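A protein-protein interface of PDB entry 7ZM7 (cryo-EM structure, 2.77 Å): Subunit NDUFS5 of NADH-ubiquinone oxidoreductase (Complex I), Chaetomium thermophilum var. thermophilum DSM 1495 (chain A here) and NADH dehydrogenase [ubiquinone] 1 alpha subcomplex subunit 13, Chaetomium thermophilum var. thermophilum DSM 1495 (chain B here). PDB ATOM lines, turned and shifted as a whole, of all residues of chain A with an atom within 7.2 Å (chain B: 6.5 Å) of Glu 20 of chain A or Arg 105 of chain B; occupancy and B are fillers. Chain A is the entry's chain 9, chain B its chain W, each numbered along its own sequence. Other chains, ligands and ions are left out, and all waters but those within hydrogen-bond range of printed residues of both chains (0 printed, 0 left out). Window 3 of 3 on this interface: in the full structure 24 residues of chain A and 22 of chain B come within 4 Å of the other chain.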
ATOM      1  N   ARG A  13      15.524   2.162  -1.381  1.00  0.00           N
ATOM      2  CA  ARG A  13      16.500   1.426  -2.237  1.00  0.00           C
ATOM      3  C   ARG A  13      16.369  -0.094  -2.144  1.00  0.00           C
ATOM      4  O   ARG A  13      16.567  -0.744  -3.174  1.00  0.00           O
ATOM      5  CB  ARG A  13      17.931   1.893  -1.953  1.00  0.00           C
ATOM      6  CG  ARG A  13      18.378   1.751  -0.509  1.00  0.00           C
ATOM      7  CD  ARG A  13      19.800   2.248  -0.356  1.00  0.00           C
ATOM      8  NE  ARG A  13      20.314   1.844   0.937  1.00  0.00           N
ATOM      9  CZ  ARG A  13      20.929   0.694   1.149  1.00  0.00           C
ATOM     10  NH1 ARG A  13      21.356   0.384   2.359  1.00  0.00           N
ATOM     11  NH2 ARG A  13      21.109  -0.142   0.145  1.00  0.00           N
ATOM     12  N   PHE A  15      13.693  -1.812  -1.192  1.00  0.00           N
ATOM     13  CA  PHE A  15      12.288  -2.288  -1.257  1.00  0.00           C
ATOM     14  C   PHE A  15      12.091  -3.315  -2.385  1.00  0.00           C
ATOM     15  O   PHE A  15      11.305  -4.241  -2.163  1.00  0.00           O
ATOM     16  CB  PHE A  15      11.351  -1.082  -1.276  1.00  0.00           C
ATOM     17  CG  PHE A  15       9.877  -1.388  -1.300  1.00  0.00           C
ATOM     18  CD1 PHE A  15       9.242  -1.871  -0.171  1.00  0.00           C
ATOM     19  CD2 PHE A  15       9.120  -1.154  -2.434  1.00  0.00           C
ATOM     20  CE1 PHE A  15       7.882  -2.125  -0.176  1.00  0.00           C
ATOM     21  CE2 PHE A  15       7.761  -1.412  -2.437  1.00  0.00           C
ATOM     22  CZ  PHE A  15       7.145  -1.894  -1.308  1.00  0.00           C
ATOM     23  N   PRO A  16      12.750  -3.244  -3.565  1.00  0.00           N
ATOM     24  CA  PRO A  16      12.581  -4.285  -4.573  1.00  0.00           C
ATOM     25  C   PRO A  16      12.986  -5.668  -4.046  1.00  0.00           C
ATOM     26  O   PRO A  16      12.256  -6.595  -4.270  1.00  0.00           O
ATOM     27  CB  PRO A  16      13.581  -3.864  -5.648  1.00  0.00           C
ATOM     28  CG  PRO A  16      13.604  -2.376  -5.566  1.00  0.00           C
ATOM     29  CD  PRO A  16      13.546  -2.124  -4.081  1.00  0.00           C
ATOM     30  N   PHE A  17      14.080  -5.752  -3.302  1.00  0.00           N
ATOM     31  CA  PHE A  17      14.565  -7.018  -2.715  1.00  0.00           C
ATOM     32  C   PHE A  17      13.565  -7.584  -1.707  1.00  0.00           C
ATOM     33  O   PHE A  17      13.421  -8.808  -1.677  1.00  0.00           O
ATOM     34  CB  PHE A  17      15.941  -6.746  -2.105  1.00  0.00           C
ATOM     35  CG  PHE A  17      16.998  -6.364  -3.107  1.00  0.00           C
ATOM     36  CD1 PHE A  17      17.190  -5.040  -3.469  1.00  0.00           C
ATOM     37  CD2 PHE A  17      17.787  -7.332  -3.702  1.00  0.00           C
ATOM     38  CE1 PHE A  17      18.157  -4.694  -4.397  1.00  0.00           C
ATOM     39  CE2 PHE A  17      18.754  -6.985  -4.629  1.00  0.00           C
ATOM     40  CZ  PHE A  17      18.940  -5.668  -4.969  1.00  0.00           C
ATOM     41  N   TRP A  18      12.946  -6.737  -0.890  1.00  0.00           N
ATOM     42  CA  TRP A  18      11.940  -7.147   0.116  1.00  0.00           C
ATOM     43  C   TRP A  18      10.690  -7.733  -0.539  1.00  0.00           C
ATOM     44  O   TRP A  18      10.144  -8.695  -0.003  1.00  0.00           O
ATOM     45  CB  TRP A  18      11.581  -5.919   0.953  1.00  0.00           C
ATOM     46  CG  TRP A  18      10.541  -6.197   1.990  1.00  0.00           C
ATOM     47  CD1 TRP A  18       9.262  -5.731   2.020  1.00  0.00           C
ATOM     48  CD2 TRP A  18      10.691  -7.043   3.140  1.00  0.00           C
ATOM     49  NE1 TRP A  18       8.610  -6.216   3.119  1.00  0.00           N
ATOM     50  CE2 TRP A  18       9.460  -7.023   3.826  1.00  0.00           C
ATOM     51  CE3 TRP A  18      11.740  -7.807   3.658  1.00  0.00           C
ATOM     52  CZ2 TRP A  18       9.254  -7.741   5.001  1.00  0.00           C
ATOM     53  CZ3 TRP A  18      11.537  -8.512   4.822  1.00  0.00           C
ATOM     54  CH2 TRP A  18      10.311  -8.477   5.481  1.00  0.00           C
ATOM     55  N   GLN A  19      10.204  -7.100  -1.598  1.00  0.00           N
ATOM     56  CA  GLN A  19       9.040  -7.624  -2.354  1.00  0.00           C
ATOM     57  C   GLN A  19       9.438  -8.910  -3.085  1.00  0.00           C
ATOM     58  O   GLN A  19       8.587  -9.782  -3.209  1.00  0.00           O
ATOM     59  CB  GLN A  19       8.440  -6.518  -3.209  1.00  0.00           C
ATOM     60  CG  GLN A  19       7.770  -5.436  -2.386  1.00  0.00           C
ATOM     61  CD  GLN A  19       6.696  -4.737  -3.178  1.00  0.00           C
ATOM     62  OE1 GLN A  19       5.593  -4.504  -2.693  1.00  0.00           O
ATOM     63  NE2 GLN A  19       7.009  -4.411  -4.420  1.00  0.00           N
ATOM     64  N   GLU A  20      10.670  -8.995  -3.578  1.00  0.00           N
ATOM     65  CA  GLU A  20      11.168 -10.237  -4.225  1.00  0.00           C
ATOM     66  C   GLU A  20      11.231 -11.336  -3.175  1.00  0.00           C
ATOM     67  O   GLU A  20      11.076 -12.495  -3.531  1.00  0.00           O
ATOM     68  CB  GLU A  20      12.501  -9.991  -4.933  1.00  0.00           C
ATOM     69  CG  GLU A  20      12.358  -9.210  -6.225  1.00  0.00           C
ATOM     70  CD  GLU A  20      13.659  -8.754  -6.860  1.00  0.00           C
ATOM     71  OE1 GLU A  20      13.773  -8.860  -8.097  1.00  0.00           O
ATOM     72  OE2 GLU A  20      14.549  -8.282  -6.124  1.00  0.00           O
ATOM     73  N   LEU A  21      11.406 -10.970  -1.913  1.00  0.00           N
ATOM     74  CA  LEU A  21      11.486 -11.944  -0.808  1.00  0.00           C
ATOM     75  C   LEU A  21      10.073 -12.231  -0.323  1.00  0.00           C
ATOM     76  O   LEU A  21       9.799 -13.391  -0.007  1.00  0.00           O
ATOM     77  CB  LEU A  21      12.312 -11.339   0.325  1.00  0.00           C
ATOM     78  CG  LEU A  21      12.406 -12.184   1.593  1.00  0.00           C
ATOM     79  CD1 LEU A  21      13.010 -13.541   1.288  1.00  0.00           C
ATOM     80  CD2 LEU A  21      13.209 -11.465   2.657  1.00  0.00           C
ATOM     81  N   LEU A  22       9.206 -11.228  -0.277  1.00  0.00           N
ATOM     82  CA  LEU A  22       7.840 -11.540   0.119  1.00  0.00           C
ATOM     83  C   LEU A  22       7.142 -12.385  -0.924  1.00  0.00           C
ATOM     84  O   LEU A  22       6.395 -13.301  -0.580  1.00  0.00           O
ATOM     85  CB  LEU A  22       7.031 -10.276   0.382  1.00  0.00           C
ATOM     86  CG  LEU A  22       7.254  -9.544   1.696  1.00  0.00           C
ATOM     87  CD1 LEU A  22       6.308  -8.373   1.788  1.00  0.00           C
ATOM     88  CD2 LEU A  22       7.068 -10.479   2.843  1.00  0.00           C
ATOM     89  N   ALA A  23       7.344 -12.069  -2.200  1.00  0.00           N
ATOM     90  CA  ALA A  23       6.705 -12.830  -3.262  1.00  0.00           C
ATOM     91  C   ALA A  23       7.174 -14.270  -3.259  1.00  0.00           C
ATOM     92  O   ALA A  23       6.365 -15.194  -3.360  1.00  0.00           O
ATOM     93  CB  ALA A  23       6.981 -12.186  -4.611  1.00  0.00           C
ATOM     94  N   CYS A  24       8.480 -14.477  -3.135  1.00  0.00           N
ATOM     95  CA  CYS A  24       9.002 -15.861  -3.030  1.00  0.00           C
ATOM     96  C   CYS A  24       8.290 -16.666  -1.937  1.00  0.00           C
ATOM     97  O   CYS A  24       7.717 -17.696  -2.287  1.00  0.00           O
ATOM     98  CB  CYS A  24      10.515 -15.852  -2.851  1.00  0.00           C
ATOM     99  SG  CYS A  24      11.309 -17.413  -3.309  1.00  0.00           S
ATOM    100  N   TYR A  25       8.307 -16.201  -0.683  1.00  0.00           N
ATOM    101  CA  TYR A  25       7.742 -16.953   0.471  1.00  0.00           C
ATOM    102  C   TYR A  25       6.256 -17.229   0.331  1.00  0.00           C
ATOM    103  O   TYR A  25       5.814 -18.298   0.731  1.00  0.00           O
ATOM    104  CB  TYR A  25       7.897 -16.146   1.759  1.00  0.00           C
ATOM    105  CG  TYR A  25       7.537 -16.876   3.028  1.00  0.00           C
ATOM    106  CD1 TYR A  25       8.418 -17.771   3.608  1.00  0.00           C
ATOM    107  CD2 TYR A  25       6.323 -16.664   3.658  1.00  0.00           C
ATOM    108  CE1 TYR A  25       8.100 -18.443   4.775  1.00  0.00           C
ATOM    109  CE2 TYR A  25       5.985 -17.332   4.823  1.00  0.00           C
ATOM    110  CZ  TYR A  25       6.878 -18.225   5.383  1.00  0.00           C
ATOM    111  OH  TYR A  25       6.561 -18.887   6.532  1.00  0.00           O
ATOM    112  N   CYS A  40      13.621 -19.220  -0.582  1.00  0.00           N
ATOM    113  CA  CYS A  40      13.690 -17.854  -0.110  1.00  0.00           C
ATOM    114  C   CYS A  40      15.016 -17.537   0.552  1.00  0.00           C
ATOM    115  O   CYS A  40      15.253 -16.378   0.894  1.00  0.00           O
ATOM    116  CB  CYS A  40      12.563 -17.610   0.890  1.00  0.00           C
ATOM    117  SG  CYS A  40      10.955 -18.061   0.302  1.00  0.00           S
ATOM    118  N   VAL A  43      17.197 -15.442  -1.703  1.00  0.00           N
ATOM    119  CA  VAL A  43      16.466 -14.198  -1.882  1.00  0.00           C
ATOM    120  C   VAL A  43      16.546 -13.351  -0.618  1.00  0.00           C
ATOM    121  O   VAL A  43      16.684 -12.127  -0.683  1.00  0.00           O
ATOM    122  CB  VAL A  43      15.017 -14.512  -2.305  1.00  0.00           C
ATOM    123  CG1 VAL A  43      14.282 -13.273  -2.742  1.00  0.00           C
ATOM    124  CG2 VAL A  43      15.029 -15.520  -3.417  1.00  0.00           C
ATOM    125  N   MET A  44      16.490 -13.992   0.551  1.00  0.00           N
ATOM    126  CA  MET A  44      16.701 -13.299   1.819  1.00  0.00           C
ATOM    127  C   MET A  44      18.128 -12.787   1.970  1.00  0.00           C
ATOM    128  O   MET A  44      18.347 -11.755   2.603  1.00  0.00           O
ATOM    129  CB  MET A  44      16.352 -14.226   2.979  1.00  0.00           C
ATOM    130  CG  MET A  44      15.795 -13.538   4.198  1.00  0.00           C
ATOM    131  SD  MET A  44      15.771 -14.535   5.692  1.00  0.00           S
ATOM    132  CE  MET A  44      17.501 -14.905   5.870  1.00  0.00           C
ATOM    133  N   ASP A  46      20.045 -11.609  -0.387  1.00  0.00           N
ATOM    134  CA  ASP A  46      20.151 -10.388  -1.162  1.00  0.00           C
ATOM    135  C   ASP A  46      19.502  -9.223  -0.442  1.00  0.00           C
ATOM    136  O   ASP A  46      20.005  -8.097  -0.493  1.00  0.00           O
ATOM    137  CB  ASP A  46      19.530 -10.584  -2.533  1.00  0.00           C
ATOM    138  CG  ASP A  46      20.152 -11.722  -3.282  1.00  0.00           C
ATOM    139  OD1 ASP A  46      21.348 -11.982  -3.068  1.00  0.00           O
ATOM    140  OD2 ASP A  46      19.448 -12.365  -4.078  1.00  0.00           O
ATOM    141  N   TYR B  83      30.576  -0.791 -15.050  1.00  0.00           N
ATOM    142  CA  TYR B  83      30.324  -2.125 -14.464  1.00  0.00           C
ATOM    143  C   TYR B  83      31.095  -3.177 -15.246  1.00  0.00           C
ATOM    144  O   TYR B  83      31.692  -4.051 -14.621  1.00  0.00           O
ATOM    145  CB  TYR B  83      28.834  -2.456 -14.434  1.00  0.00           C
ATOM    146  CG  TYR B  83      28.528  -3.884 -14.061  1.00  0.00           C
ATOM    147  CD1 TYR B  83      28.402  -4.259 -12.737  1.00  0.00           C
ATOM    148  CD2 TYR B  83      28.389  -4.865 -15.027  1.00  0.00           C
ATOM    149  CE1 TYR B  83      28.141  -5.569 -12.381  1.00  0.00           C
ATOM    150  CE2 TYR B  83      28.130  -6.180 -14.690  1.00  0.00           C
ATOM    151  CZ  TYR B  83      28.004  -6.533 -13.362  1.00  0.00           C
ATOM    152  OH  TYR B  83      27.741  -7.828 -13.021  1.00  0.00           O
ATOM    153  N   LYS B  99      30.655 -13.137  -6.591  1.00  0.00           N
ATOM    154  CA  LYS B  99      29.236 -12.715  -6.793  1.00  0.00           C
ATOM    155  C   LYS B  99      28.667 -12.172  -5.479  1.00  0.00           C
ATOM    156  O   LYS B  99      28.673 -12.916  -4.486  1.00  0.00           O
ATOM    157  CB  LYS B  99      28.438 -13.930  -7.273  1.00  0.00           C
ATOM    158  CG  LYS B  99      27.098 -13.633  -7.927  1.00  0.00           C
ATOM    159  CD  LYS B  99      27.196 -12.908  -9.250  1.00  0.00           C
ATOM    160  CE  LYS B  99      25.853 -12.412  -9.742  1.00  0.00           C
ATOM    161  NZ  LYS B  99      24.794 -13.438  -9.585  1.00  0.00           N
ATOM    162  N   TYR B 101      25.560 -10.717  -5.093  1.00  0.00           N
ATOM    163  CA  TYR B 101      24.099 -10.940  -5.047  1.00  0.00           C
ATOM    164  C   TYR B 101      23.820 -12.253  -5.772  1.00  0.00           C
ATOM    165  O   TYR B 101      24.566 -12.599  -6.665  1.00  0.00           O
ATOM    166  CB  TYR B 101      23.395  -9.749  -5.687  1.00  0.00           C
ATOM    167  CG  TYR B 101      23.301  -8.531  -4.807  1.00  0.00           C
ATOM    168  CD1 TYR B 101      22.245  -8.370  -3.928  1.00  0.00           C
ATOM    169  CD2 TYR B 101      24.270  -7.546  -4.847  1.00  0.00           C
ATOM    170  CE1 TYR B 101      22.152  -7.257  -3.112  1.00  0.00           C
ATOM    171  CE2 TYR B 101      24.199  -6.434  -4.028  1.00  0.00           C
ATOM    172  CZ  TYR B 101      23.128  -6.283  -3.169  1.00  0.00           C
ATOM    173  OH  TYR B 101      23.048  -5.186  -2.370  1.00  0.00           O
ATOM    174  N   SER B 103      21.349 -12.799  -7.726  1.00  0.00           N
ATOM    175  CA  SER B 103      20.371 -12.397  -8.768  1.00  0.00           C
ATOM    176  C   SER B 103      21.103 -11.671  -9.905  1.00  0.00           C
ATOM    177  O   SER B 103      22.224 -11.182  -9.660  1.00  0.00           O
ATOM    178  CB  SER B 103      19.292 -11.537  -8.194  1.00  0.00           C
ATOM    179  OG  SER B 103      19.832 -10.539  -7.345  1.00  0.00           O
ATOM    180  N   ASP B 104      20.497 -11.610 -11.095  1.00  0.00           N
ATOM    181  CA  ASP B 104      21.126 -10.952 -12.278  1.00  0.00           C
ATOM    182  C   ASP B 104      20.886  -9.444 -12.204  1.00  0.00           C
ATOM    183  O   ASP B 104      21.464  -8.730 -13.019  1.00  0.00           O
ATOM    184  CB  ASP B 104      20.619 -11.538 -13.596  1.00  0.00           C
ATOM    185  CG  ASP B 104      19.114 -11.451 -13.789  1.00  0.00           C
ATOM    186  OD1 ASP B 104      18.406 -11.144 -12.809  1.00  0.00           O
ATOM    187  OD2 ASP B 104      18.659 -11.689 -14.925  1.00  0.00           O
ATOM    188  N   ARG B 105      20.127  -8.995 -11.224  1.00  0.00           N
ATOM    189  CA  ARG B 105      19.824  -7.565 -11.049  1.00  0.00           C
ATOM    190  C   ARG B 105      21.106  -6.748 -11.026  1.00  0.00           C
ATOM    191  O   ARG B 105      22.095  -7.219 -10.444  1.00  0.00           O
ATOM    192  CB  ARG B 105      19.093  -7.335  -9.728  1.00  0.00           C
ATOM    193  CG  ARG B 105      17.634  -7.763  -9.749  1.00  0.00           C
ATOM    194  CD  ARG B 105      17.008  -7.548  -8.387  1.00  0.00           C
ATOM    195  NE  ARG B 105      17.101  -6.154  -7.982  1.00  0.00           N
ATOM    196  CZ  ARG B 105      16.151  -5.252  -8.168  1.00  0.00           C
ATOM    197  NH1 ARG B 105      16.339  -4.010  -7.763  1.00  0.00           N
ATOM    198  NH2 ARG B 105      15.014  -5.589  -8.749  1.00  0.00           N
ATOM    199  N   TYR B 106      21.086  -5.574 -11.636  1.00  0.00           N
ATOM    200  CA  TYR B 106      22.246  -4.673 -11.517  1.00  0.00           C
ATOM    201  C   TYR B 106      21.987  -3.834 -10.275  1.00  0.00           C
ATOM    202  O   TYR B 106      20.957  -3.167 -10.191  1.00  0.00           O
ATOM    203  CB  TYR B 106      22.398  -3.781 -12.752  1.00  0.00           C
ATOM    204  CG  TYR B 106      23.288  -2.593 -12.506  1.00  0.00           C
ATOM    205  CD1 TYR B 106      24.634  -2.765 -12.234  1.00  0.00           C
ATOM    206  CD2 TYR B 106      22.776  -1.309 -12.498  1.00  0.00           C
ATOM    207  CE1 TYR B 106      25.456  -1.685 -11.971  1.00  0.00           C
ATOM    208  CE2 TYR B 106      23.583  -0.218 -12.239  1.00  0.00           C
ATOM    209  CZ  TYR B 106      24.925  -0.411 -11.980  1.00  0.00           C
ATOM    210  OH  TYR B 106      25.721   0.661 -11.719  1.00  0.00           O
ATOM    211  N   VAL B 107      22.951  -3.924  -9.319  1.00  0.00           N
ATOM    212  CA  VAL B 107      22.822  -3.081  -8.103  1.00  0.00           C
ATOM    213  C   VAL B 107      23.798  -1.923  -8.263  1.00  0.00           C
ATOM    214  O   VAL B 107      24.898  -2.188  -8.649  1.00  0.00           O
ATOM    215  CB  VAL B 107      23.056  -3.904  -6.819  1.00  0.00           C
ATOM    216  CG1 VAL B 107      22.694  -3.108  -5.580  1.00  0.00           C
ATOM    217  CG2 VAL B 107      22.269  -5.203  -6.861  1.00  0.00           C
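Of the 16 printed residues of chain A, 4 touch a printed residue of chain B.
Printed residues of chain A that touch a printed residue of chain B: Pro 16, Phe 17, Glu 20 and Asp 46.
Hydrophobic or aromatic side chains of chain A within 4 Å of the printed part of chain B: Pro 16 and Phe 17.
Of the 8 printed residues of chain B, 4 touch a printed residue of chain A.
Hydrophobic or aromatic side chains of chain B that line the printed part of chain A: Tyr 101 and Val 107.
Along chain B the printed residues that touch a printed residue of chain A span positions 101 to 107.
Among the printed residues, 7 pairs touch across the chains.
Among the printed residues, merely in contact across the chains: Pro 16 of chain A with Arg 105 of chain B, Phe 17 of chain A with Tyr 101 of chain B, Phe 17 of chain A with Arg 105 of chain B, Phe 17 of chain A with Val 107 of chain B, Asp 46 of chain A with Tyr 101 of chain B and Asp 46 of chain A with Ser 103 of chain B.
Printed residues of chain A within 4 Å of Arg 105 of chain B: Pro 16, Phe 17 and Glu 20.
Printed residues of chain A within 4 Å of Tyr 101 of chain B: Phe 17 and Asp 46.
Of the printed residues of chain A, Ser 103 of chain B touches Asp 46.
Of the printed residues of chain B, Phe 17 of chain A touches Tyr 101 (3.7 Å), Arg 105 (3.6 Å) and Val 107 (3.9 Å).
Of the printed residues of chain A, Val 107 of chain B touches Phe 17 (3.9 Å).
Printed residues of chain B within 4 Å of Asp 46 of chain A: Tyr 101 and Ser 103.
Phe 15 of chain A touches none of the printed residues of chain B.
Tyr 83 of chain B touches none of the printed residues of chain A.
The nearest residue of chain A that does not touch Arg 105 of chain B is Arg 13 of chain A (5.6 Å).
The guanidinium group (NH2) of Arg 105 of chain B lies within salt-bridge range of the side-chain carboxylate (OE1) of Glu 20 of chain A (3.6 Å).
NZ of Lys 99 of chain B is in hydrogen-bond range of O of Ser 103 of chain B (3.4 Å).
The side-chain amino group (NZ) of Lys 99 of chain B lies close to the backbone carbonyl oxygen (O) of Tyr 101 of chain B (3.0 Å).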
